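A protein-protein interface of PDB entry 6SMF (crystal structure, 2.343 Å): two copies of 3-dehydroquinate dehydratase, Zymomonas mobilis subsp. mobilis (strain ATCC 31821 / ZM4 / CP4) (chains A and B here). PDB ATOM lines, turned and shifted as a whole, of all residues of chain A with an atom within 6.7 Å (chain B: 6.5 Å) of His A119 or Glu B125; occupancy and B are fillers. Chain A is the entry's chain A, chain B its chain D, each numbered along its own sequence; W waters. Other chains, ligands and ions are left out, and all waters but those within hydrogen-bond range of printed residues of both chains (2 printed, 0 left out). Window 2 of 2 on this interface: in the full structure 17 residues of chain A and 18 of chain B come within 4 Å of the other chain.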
ATOM      1  N   HIS A  87      -4.004   6.978   8.970  1.00  0.00           N
ATOM      2  CA  HIS A  87      -2.574   6.986   8.601  1.00  0.00           C
ATOM      3  C   HIS A  87      -1.699   6.463   9.743  1.00  0.00           C
ATOM      4  O   HIS A  87      -0.532   6.171   9.460  1.00  0.00           O
ATOM      5  CB  HIS A  87      -2.149   8.381   8.122  1.00  0.00           C
ATOM      6  CG  HIS A  87      -3.171   9.019   7.245  1.00  0.00           C
ATOM      7  ND1 HIS A  87      -3.656   8.400   6.083  1.00  0.00           N
ATOM      8  CD2 HIS A  87      -3.869  10.162   7.403  1.00  0.00           C
ATOM      9  CE1 HIS A  87      -4.611   9.136   5.559  1.00  0.00           C
ATOM     10  NE2 HIS A  87      -4.770  10.235   6.353  1.00  0.00           N
ATOM     11  N   ASN A 110      -9.557  13.777  -1.231  1.00  0.00           N
ATOM     12  CA  ASN A 110      -8.738  12.693  -1.805  1.00  0.00           C
ATOM     13  C   ASN A 110      -7.401  12.726  -1.075  1.00  0.00           C
ATOM     14  O   ASN A 110      -6.572  13.605  -1.325  1.00  0.00           O
ATOM     15  CB  ASN A 110      -8.608  12.872  -3.322  1.00  0.00           C
ATOM     16  CG  ASN A 110      -7.661  11.888  -3.984  1.00  0.00           C
ATOM     17  OD1 ASN A 110      -7.113  10.985  -3.338  1.00  0.00           O
ATOM     18  ND2 ASN A 110      -7.471  12.075  -5.285  1.00  0.00           N
ATOM     19  N   PRO A 111      -7.141  11.791  -0.149  1.00  0.00           N
ATOM     20  CA  PRO A 111      -5.921  11.857   0.647  1.00  0.00           C
ATOM     21  C   PRO A 111      -4.646  11.695  -0.208  1.00  0.00           C
ATOM     22  O   PRO A 111      -3.634  12.195   0.183  1.00  0.00           O
ATOM     23  CB  PRO A 111      -6.061  10.733   1.675  1.00  0.00           C
ATOM     24  CG  PRO A 111      -7.214   9.873   1.217  1.00  0.00           C
ATOM     25  CD  PRO A 111      -7.988  10.657   0.189  1.00  0.00           C
ATOM     26  N   HIS A 112      -4.712  11.016  -1.352  1.00  0.00           N
ATOM     27  CA  HIS A 112      -3.553  10.793  -2.246  1.00  0.00           C
ATOM     28  C   HIS A 112      -3.181  12.138  -2.870  1.00  0.00           C
ATOM     29  O   HIS A 112      -2.010  12.270  -3.304  1.00  0.00           O
ATOM     30  CB  HIS A 112      -3.830   9.675  -3.299  1.00  0.00           C
ATOM     31  CG  HIS A 112      -3.686   8.288  -2.759  1.00  0.00           C
ATOM     32  ND1 HIS A 112      -2.542   7.534  -2.960  1.00  0.00           N
ATOM     33  CD2 HIS A 112      -4.498   7.544  -1.971  1.00  0.00           C
ATOM     34  CE1 HIS A 112      -2.670   6.387  -2.323  1.00  0.00           C
ATOM     35  NE2 HIS A 112      -3.847   6.372  -1.709  1.00  0.00           N
ATOM     36  N   ALA A 113      -4.106  13.114  -2.875  1.00  0.00           N
ATOM     37  CA  ALA A 113      -3.854  14.445  -3.475  1.00  0.00           C
ATOM     38  C   ALA A 113      -3.200  15.366  -2.432  1.00  0.00           C
ATOM     39  O   ALA A 113      -2.940  16.498  -2.740  1.00  0.00           O
ATOM     40  CB  ALA A 113      -5.129  15.036  -4.030  1.00  0.00           C
ATOM     41  N   ARG A 114      -2.961  14.876  -1.234  1.00  0.00           N
ATOM     42  CA  ARG A 114      -2.466  15.705  -0.122  1.00  0.00           C
ATOM     43  C   ARG A 114      -1.026  15.297   0.233  1.00  0.00           C
ATOM     44  O   ARG A 114      -0.308  14.754  -0.662  1.00  0.00           O
ATOM     45  CB  ARG A 114      -3.521  15.584   0.987  1.00  0.00           C
ATOM     46  CG  ARG A 114      -4.869  16.168   0.555  1.00  0.00           C
ATOM     47  CD  ARG A 114      -5.973  16.059   1.558  1.00  0.00           C
ATOM     48  NE  ARG A 114      -5.696  16.906   2.712  1.00  0.00           N
ATOM     49  CZ  ARG A 114      -6.333  16.868   3.863  1.00  0.00           C
ATOM     50  NH1 ARG A 114      -5.929  17.669   4.825  1.00  0.00           N
ATOM     51  NH2 ARG A 114      -7.342  16.043   4.051  1.00  0.00           N
ATOM     52  N   GLU A 115      -0.607  15.630   1.452  1.00  0.00           N
ATOM     53  CA  GLU A 115       0.715  15.299   2.050  1.00  0.00           C
ATOM     54  C   GLU A 115       0.933  13.796   1.879  1.00  0.00           C
ATOM     55  O   GLU A 115      -0.070  12.995   2.063  1.00  0.00           O
ATOM     56  CB  GLU A 115       0.731  15.677   3.561  1.00  0.00           C
ATOM     57  CG  GLU A 115       0.203  17.091   3.882  1.00  0.00           C
ATOM     58  CD  GLU A 115      -1.146  17.176   4.589  1.00  0.00           C
ATOM     59  OE1 GLU A 115      -1.227  17.865   5.704  1.00  0.00           O
ATOM     60  OE2 GLU A 115      -2.135  16.551   4.058  1.00  0.00           O
ATOM     61  N   ALA A 116       2.172  13.424   1.565  1.00  0.00           N
ATOM     62  CA  ALA A 116       2.674  12.025   1.438  1.00  0.00           C
ATOM     63  C   ALA A 116       2.285  11.196   2.671  1.00  0.00           C
ATOM     64  O   ALA A 116       1.919  10.030   2.483  1.00  0.00           O
ATOM     65  CB  ALA A 116       4.169  12.050   1.282  1.00  0.00           C
ATOM     66  N   PHE A 117       2.290  11.757   3.892  1.00  0.00           N
ATOM     67  CA  PHE A 117       1.951  10.926   5.062  1.00  0.00           C
ATOM     68  C   PHE A 117       0.490  10.490   4.971  1.00  0.00           C
ATOM     69  O   PHE A 117       0.147   9.579   5.680  1.00  0.00           O
ATOM     70  CB  PHE A 117       2.251  11.553   6.418  1.00  0.00           C
ATOM     71  CG  PHE A 117       1.459  12.773   6.818  1.00  0.00           C
ATOM     72  CD1 PHE A 117       0.179  12.655   7.324  1.00  0.00           C
ATOM     73  CD2 PHE A 117       1.995  14.033   6.682  1.00  0.00           C
ATOM     74  CE1 PHE A 117      -0.577  13.780   7.594  1.00  0.00           C
ATOM     75  CE2 PHE A 117       1.257  15.150   6.996  1.00  0.00           C
ATOM     76  CZ  PHE A 117      -0.019  15.020   7.481  1.00  0.00           C
ATOM     77  N   ARG A 118      -0.369  11.125   4.197  1.00  0.00           N
ATOM     78  CA  ARG A 118      -1.787  10.670   4.092  1.00  0.00           C
ATOM     79  C   ARG A 118      -1.954   9.603   3.003  1.00  0.00           C
ATOM     80  O   ARG A 118      -3.041   9.107   2.880  1.00  0.00           O
ATOM     81  CB  ARG A 118      -2.707  11.837   3.753  1.00  0.00           C
ATOM     82  CG  ARG A 118      -2.690  12.959   4.776  1.00  0.00           C
ATOM     83  CD  ARG A 118      -3.931  13.837   4.603  1.00  0.00           C
ATOM     84  NE  ARG A 118      -3.625  15.087   5.287  1.00  0.00           N
ATOM     85  CZ  ARG A 118      -3.930  15.354   6.557  1.00  0.00           C
ATOM     86  NH1 ARG A 118      -4.650  14.503   7.282  1.00  0.00           N
ATOM     87  NH2 ARG A 118      -3.486  16.479   7.080  1.00  0.00           N
ATOM     88  N   HIS A 119      -0.905   9.287   2.222  1.00  0.00           N
ATOM     89  CA  HIS A 119      -0.941   8.199   1.217  1.00  0.00           C
ATOM     90  C   HIS A 119      -1.098   6.846   1.912  1.00  0.00           C
ATOM     91  O   HIS A 119      -1.674   5.951   1.321  1.00  0.00           O
ATOM     92  CB  HIS A 119       0.269   8.280   0.333  1.00  0.00           C
ATOM     93  CG  HIS A 119       0.295   9.525  -0.476  1.00  0.00           C
ATOM     94  ND1 HIS A 119       1.295   9.785  -1.392  1.00  0.00           N
ATOM     95  CD2 HIS A 119      -0.527  10.602  -0.468  1.00  0.00           C
ATOM     96  CE1 HIS A 119       1.066  10.964  -1.923  1.00  0.00           C
ATOM     97  NE2 HIS A 119      -0.061  11.473  -1.396  1.00  0.00           N
ATOM     98  N   LYS A 120      -0.664   6.722   3.164  1.00  0.00           N
ATOM     99  CA  LYS A 120      -0.746   5.459   3.915  1.00  0.00           C
ATOM    100  C   LYS A 120      -2.149   5.312   4.494  1.00  0.00           C
ATOM    101  O   LYS A 120      -2.602   6.208   5.201  1.00  0.00           O
ATOM    102  CB  LYS A 120       0.314   5.492   5.004  1.00  0.00           C
ATOM    103  CG  LYS A 120       0.288   4.313   5.960  1.00  0.00           C
ATOM    104  CD  LYS A 120       0.800   3.065   5.289  1.00  0.00           C
ATOM    105  CE  LYS A 120       0.980   1.902   6.272  1.00  0.00           C
ATOM    106  NZ  LYS A 120       1.479   0.687   5.565  1.00  0.00           N
ATOM    107  N   SER A 121      -2.808   4.200   4.235  1.00  0.00           N
ATOM    108  CA  SER A 121      -4.135   3.947   4.823  1.00  0.00           C
ATOM    109  C   SER A 121      -4.188   2.562   5.497  1.00  0.00           C
ATOM    110  O   SER A 121      -4.377   1.543   4.806  1.00  0.00           O
ATOM    111  CB  SER A 121      -5.184   4.116   3.799  1.00  0.00           C
ATOM    112  OG  SER A 121      -6.415   3.870   4.418  1.00  0.00           O
ATOM    113  N   TYR B  93      -0.448  10.890 -14.633  1.00  0.00           N
ATOM    114  CA  TYR B  93      -0.613  11.896 -13.559  1.00  0.00           C
ATOM    115  C   TYR B  93      -0.639  13.278 -14.205  1.00  0.00           C
ATOM    116  O   TYR B  93      -1.540  14.077 -13.884  1.00  0.00           O
ATOM    117  CB  TYR B  93       0.464  11.739 -12.484  1.00  0.00           C
ATOM    118  CG  TYR B  93       0.681  12.939 -11.600  1.00  0.00           C
ATOM    119  CD1 TYR B  93      -0.037  13.109 -10.418  1.00  0.00           C
ATOM    120  CD2 TYR B  93       1.629  13.894 -11.916  1.00  0.00           C
ATOM    121  CE1 TYR B  93       0.187  14.195  -9.581  1.00  0.00           C
ATOM    122  CE2 TYR B  93       1.904  14.954 -11.070  1.00  0.00           C
ATOM    123  CZ  TYR B  93       1.172  15.116  -9.909  1.00  0.00           C
ATOM    124  OH  TYR B  93       1.408  16.213  -9.145  1.00  0.00           O
ATOM    125  N   ARG B  97      -3.756  16.080 -14.581  1.00  0.00           N
ATOM    126  CA  ARG B  97      -3.561  17.454 -14.088  1.00  0.00           C
ATOM    127  C   ARG B  97      -3.701  18.491 -15.207  1.00  0.00           C
ATOM    128  O   ARG B  97      -4.187  19.596 -14.890  1.00  0.00           O
ATOM    129  CB  ARG B  97      -2.245  17.547 -13.333  1.00  0.00           C
ATOM    130  CG  ARG B  97      -2.417  17.004 -11.929  1.00  0.00           C
ATOM    131  CD  ARG B  97      -1.232  17.252 -11.047  1.00  0.00           C
ATOM    132  NE  ARG B  97      -1.382  18.494 -10.290  1.00  0.00           N
ATOM    133  CZ  ARG B  97      -0.425  19.405 -10.167  1.00  0.00           C
ATOM    134  NH1 ARG B  97       0.751  19.227 -10.745  1.00  0.00           N
ATOM    135  NH2 ARG B  97      -0.627  20.510  -9.474  1.00  0.00           N
ATOM    136  N   GLU B 105     -10.832   7.763 -10.292  1.00  0.00           N
ATOM    137  CA  GLU B 105     -10.045   6.526 -10.264  1.00  0.00           C
ATOM    138  C   GLU B 105     -10.979   5.390  -9.883  1.00  0.00           C
ATOM    139  O   GLU B 105     -11.729   5.553  -8.930  1.00  0.00           O
ATOM    140  CB  GLU B 105      -8.895   6.650  -9.280  1.00  0.00           C
ATOM    141  CG  GLU B 105      -7.871   5.535  -9.373  1.00  0.00           C
ATOM    142  CD  GLU B 105      -6.753   5.637  -8.338  1.00  0.00           C
ATOM    143  OE1 GLU B 105      -6.829   6.516  -7.444  1.00  0.00           O
ATOM    144  OE2 GLU B 105      -5.805   4.803  -8.394  1.00  0.00           O
ATOM    145  N   HIS B 112      -4.854  -1.302  -1.802  1.00  0.00           N
ATOM    146  CA  HIS B 112      -4.176  -1.120  -0.490  1.00  0.00           C
ATOM    147  C   HIS B 112      -4.172  -2.471   0.204  1.00  0.00           C
ATOM    148  O   HIS B 112      -3.346  -2.646   1.091  1.00  0.00           O
ATOM    149  CB  HIS B 112      -4.788   0.009   0.373  1.00  0.00           C
ATOM    150  CG  HIS B 112      -4.466   1.399  -0.076  1.00  0.00           C
ATOM    151  ND1 HIS B 112      -3.475   2.159   0.531  1.00  0.00           N
ATOM    152  CD2 HIS B 112      -4.972   2.144  -1.083  1.00  0.00           C
ATOM    153  CE1 HIS B 112      -3.381   3.321  -0.091  1.00  0.00           C
ATOM    154  NE2 HIS B 112      -4.278   3.328  -1.102  1.00  0.00           N
ATOM    155  N   HIS B 119       0.175   0.260  -3.443  1.00  0.00           N
ATOM    156  CA  HIS B 119      -0.253   1.368  -2.551  1.00  0.00           C
ATOM    157  C   HIS B 119      -0.061   2.725  -3.247  1.00  0.00           C
ATOM    158  O   HIS B 119      -0.804   3.628  -2.962  1.00  0.00           O
ATOM    159  CB  HIS B 119       0.462   1.264  -1.230  1.00  0.00           C
ATOM    160  CG  HIS B 119       0.064   0.035  -0.481  1.00  0.00           C
ATOM    161  ND1 HIS B 119       0.559  -0.252   0.779  1.00  0.00           N
ATOM    162  CD2 HIS B 119      -0.718  -1.016  -0.850  1.00  0.00           C
ATOM    163  CE1 HIS B 119       0.096  -1.417   1.135  1.00  0.00           C
ATOM    164  NE2 HIS B 119      -0.703  -1.897   0.146  1.00  0.00           N
ATOM    165  N   LYS B 120       0.873   2.812  -4.179  1.00  0.00           N
ATOM    166  CA  LYS B 120       1.249   4.058  -4.871  1.00  0.00           C
ATOM    167  C   LYS B 120       0.276   4.316  -6.006  1.00  0.00           C
ATOM    168  O   LYS B 120       0.103   3.396  -6.851  1.00  0.00           O
ATOM    169  CB  LYS B 120       2.671   3.924  -5.410  1.00  0.00           C
ATOM    170  CG  LYS B 120       3.160   5.105  -6.207  1.00  0.00           C
ATOM    171  CD  LYS B 120       3.397   6.335  -5.370  1.00  0.00           C
ATOM    172  CE  LYS B 120       3.864   7.491  -6.229  1.00  0.00           C
ATOM    173  NZ  LYS B 120       4.181   8.654  -5.375  1.00  0.00           N
ATOM    174  N   SER B 121      -0.356   5.486  -6.028  1.00  0.00           N
ATOM    175  CA  SER B 121      -1.292   5.760  -7.142  1.00  0.00           C
ATOM    176  C   SER B 121      -1.015   7.122  -7.768  1.00  0.00           C
ATOM    177  O   SER B 121      -1.446   8.122  -7.238  1.00  0.00           O
ATOM    178  CB  SER B 121      -2.706   5.598  -6.702  1.00  0.00           C
ATOM    179  OG  SER B 121      -3.560   5.912  -7.776  1.00  0.00           O
ATOM    180  N   TYR B 122      -0.324   7.143  -8.885  1.00  0.00           N
ATOM    181  CA  TYR B 122      -0.106   8.396  -9.662  1.00  0.00           C
ATOM    182  C   TYR B 122      -1.469   8.908 -10.122  1.00  0.00           C
ATOM    183  O   TYR B 122      -1.718  10.079 -10.045  1.00  0.00           O
ATOM    184  CB  TYR B 122       0.897   8.165 -10.799  1.00  0.00           C
ATOM    185  CG  TYR B 122       2.337   8.151 -10.368  1.00  0.00           C
ATOM    186  CD1 TYR B 122       2.957   9.290  -9.900  1.00  0.00           C
ATOM    187  CD2 TYR B 122       3.071   6.985 -10.387  1.00  0.00           C
ATOM    188  CE1 TYR B 122       4.280   9.295  -9.490  1.00  0.00           C
ATOM    189  CE2 TYR B 122       4.376   6.960  -9.935  1.00  0.00           C
ATOM    190  CZ  TYR B 122       4.996   8.126  -9.526  1.00  0.00           C
ATOM    191  OH  TYR B 122       6.312   8.118  -9.121  1.00  0.00           O
ATOM    192  N   VAL B 123      -2.390   8.037 -10.467  1.00  0.00           N
ATOM    193  CA  VAL B 123      -3.778   8.483 -10.825  1.00  0.00           C
ATOM    194  C   VAL B 123      -4.426   9.195  -9.639  1.00  0.00           C
ATOM    195  O   VAL B 123      -4.897  10.355  -9.795  1.00  0.00           O
ATOM    196  CB  VAL B 123      -4.646   7.316 -11.297  1.00  0.00           C
ATOM    197  CG1 VAL B 123      -6.080   7.753 -11.420  1.00  0.00           C
ATOM    198  CG2 VAL B 123      -4.132   6.804 -12.624  1.00  0.00           C
ATOM    199  N   GLY B 124      -4.440   8.504  -8.499  1.00  0.00           N
ATOM    200  CA  GLY B 124      -5.069   9.017  -7.273  1.00  0.00           C
ATOM    201  C   GLY B 124      -4.465  10.347  -6.836  1.00  0.00           C
ATOM    202  O   GLY B 124      -5.202  11.150  -6.236  1.00  0.00           O
ATOM    203  N   GLU B 125      -3.182  10.570  -7.092  1.00  0.00           N
ATOM    204  CA  GLU B 125      -2.511  11.819  -6.696  1.00  0.00           C
ATOM    205  C   GLU B 125      -3.057  13.007  -7.516  1.00  0.00           C
ATOM    206  O   GLU B 125      -2.854  14.132  -7.073  1.00  0.00           O
ATOM    207  CB  GLU B 125      -0.993  11.690  -6.850  1.00  0.00           C
ATOM    208  CG  GLU B 125      -0.418  10.839  -5.777  1.00  0.00           C
ATOM    209  CD  GLU B 125       1.071  10.597  -5.821  1.00  0.00           C
ATOM    210  OE1 GLU B 125       1.819  11.518  -6.321  1.00  0.00           O
ATOM    211  OE2 GLU B 125       1.455   9.475  -5.312  1.00  0.00           O
ATOM    212  N   ALA B 126      -3.698  12.768  -8.659  1.00  0.00           N
ATOM    213  CA  ALA B 126      -4.127  13.843  -9.571  1.00  0.00           C
ATOM    214  C   ALA B 126      -5.649  13.879  -9.740  1.00  0.00           C
ATOM    215  O   ALA B 126      -6.158  14.868 -10.236  1.00  0.00           O
ATOM    216  CB  ALA B 126      -3.435  13.594 -10.891  1.00  0.00           C
ATOM    217  N   ALA B 127      -6.336  12.790  -9.441  1.00  0.00           N
ATOM    218  CA  ALA B 127      -7.783  12.608  -9.679  1.00  0.00           C
ATOM    219  C   ALA B 127      -8.608  13.362  -8.634  1.00  0.00           C
ATOM    220  O   ALA B 127      -8.074  13.833  -7.610  1.00  0.00           O
ATOM    221  CB  ALA B 127      -8.124  11.138  -9.651  1.00  0.00           C
HETATM  222  O   HOH W   1      -1.463   1.978   2.652  1.00  0.00           O
HETATM  223  O   HOH W   2       0.273   7.601  -3.992  1.00  0.00           O
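Hydrophobic or aromatic side chains of chain B within 4 Å of the printed part of chain A: His B112.
Of the 13 printed residues of chain A, 4 touch a printed residue of chain B.
Printed residues of chain A that touch a printed residue of chain B: Asn A110, His A112, Ala A113 and His A119.
Hydrophobic or aromatic side chains of chain A within 4 Å of the printed part of chain B: His A112, Ala A113 and His A119.
Among the printed residues, no Asp or Glu carboxylate lies within 4 Å of a Lys or Arg side-chain nitrogen of the other chain.
NE2 of His A112 lies within hydrogen-bond range of NE2 of His B112 (3.1 Å).
The side-chain amide nitrogen (ND2) of Asn A110 sits at hydrogen-bond distance from the backbone carbonyl oxygen (O) of Gly B124, 2.6 Å away.
O of Ala B127 lies within hydrogen-bond range of ND2 of Asn A110 (3.0 Å).
Water W2 lies within hydrogen-bond range of OE2 of Glu B125 (2.6 Å), ND1 of His A112 (3.0 Å) and N of Ser B121 (3.0 Å).
Water W1 bridges a ring nitrogen (ND1) of His B112 and the backbone NH of Ser A121.
Among the printed residues, merely in contact across the chains: His A112 with Glu B125, His A112 with His B119, His A119 with His B112, His A112 with Gly B124, His A119 with Glu B125 and Ala A113 with Glu B125.
NZ of Lys B120 lies within salt-bridge range of OE2 of Glu B125 (2.8 Å).
The side-chain carboxylate (OE1) of Glu B105 sits close to the backbone NH (N) of Gly B124, at 3.3 Å.
O of Arg A114 is in hydrogen-bond range of NE2 of His A119.
The backbone NH (N) of Gly B124 sits at hydrogen-bond distance from the side-chain hydroxyl (OG) of Ser B121, 2.8 Å away.
O of His A112 is in hydrogen-bond range of NE2 of His A119, at 2.8 Å.
NE2 of His B119 is in hydrogen-bond range of O of His B112.
His B112 touches its own counterpart, His A112.
His A112 touches His B119, and with the chains exchanged His A119 touches His B112.
Of the 9 pairs that touch across the chains among the printed residues, 3 have their exchanged pair printed and touching as well.
Of chain A, only His A112 (3.3 Å), Ala A113 (3.7 Å) and His A119 (3.7 Å) come within 4 Å of Glu B125.
Of the printed residues of chain A, Ala B127 touches Asn A110 (3.0 Å).
Of the printed residues of chain A, His B112 touches His A112 (3.1 Å) and His A119 (3.4 Å).
The nearest residue of chain B that does not touch His A119 is His B119 (4.9 Å).
The nearest printed residue of chain A that does not touch Gly B124 is Ala A113 (4.04 Å).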
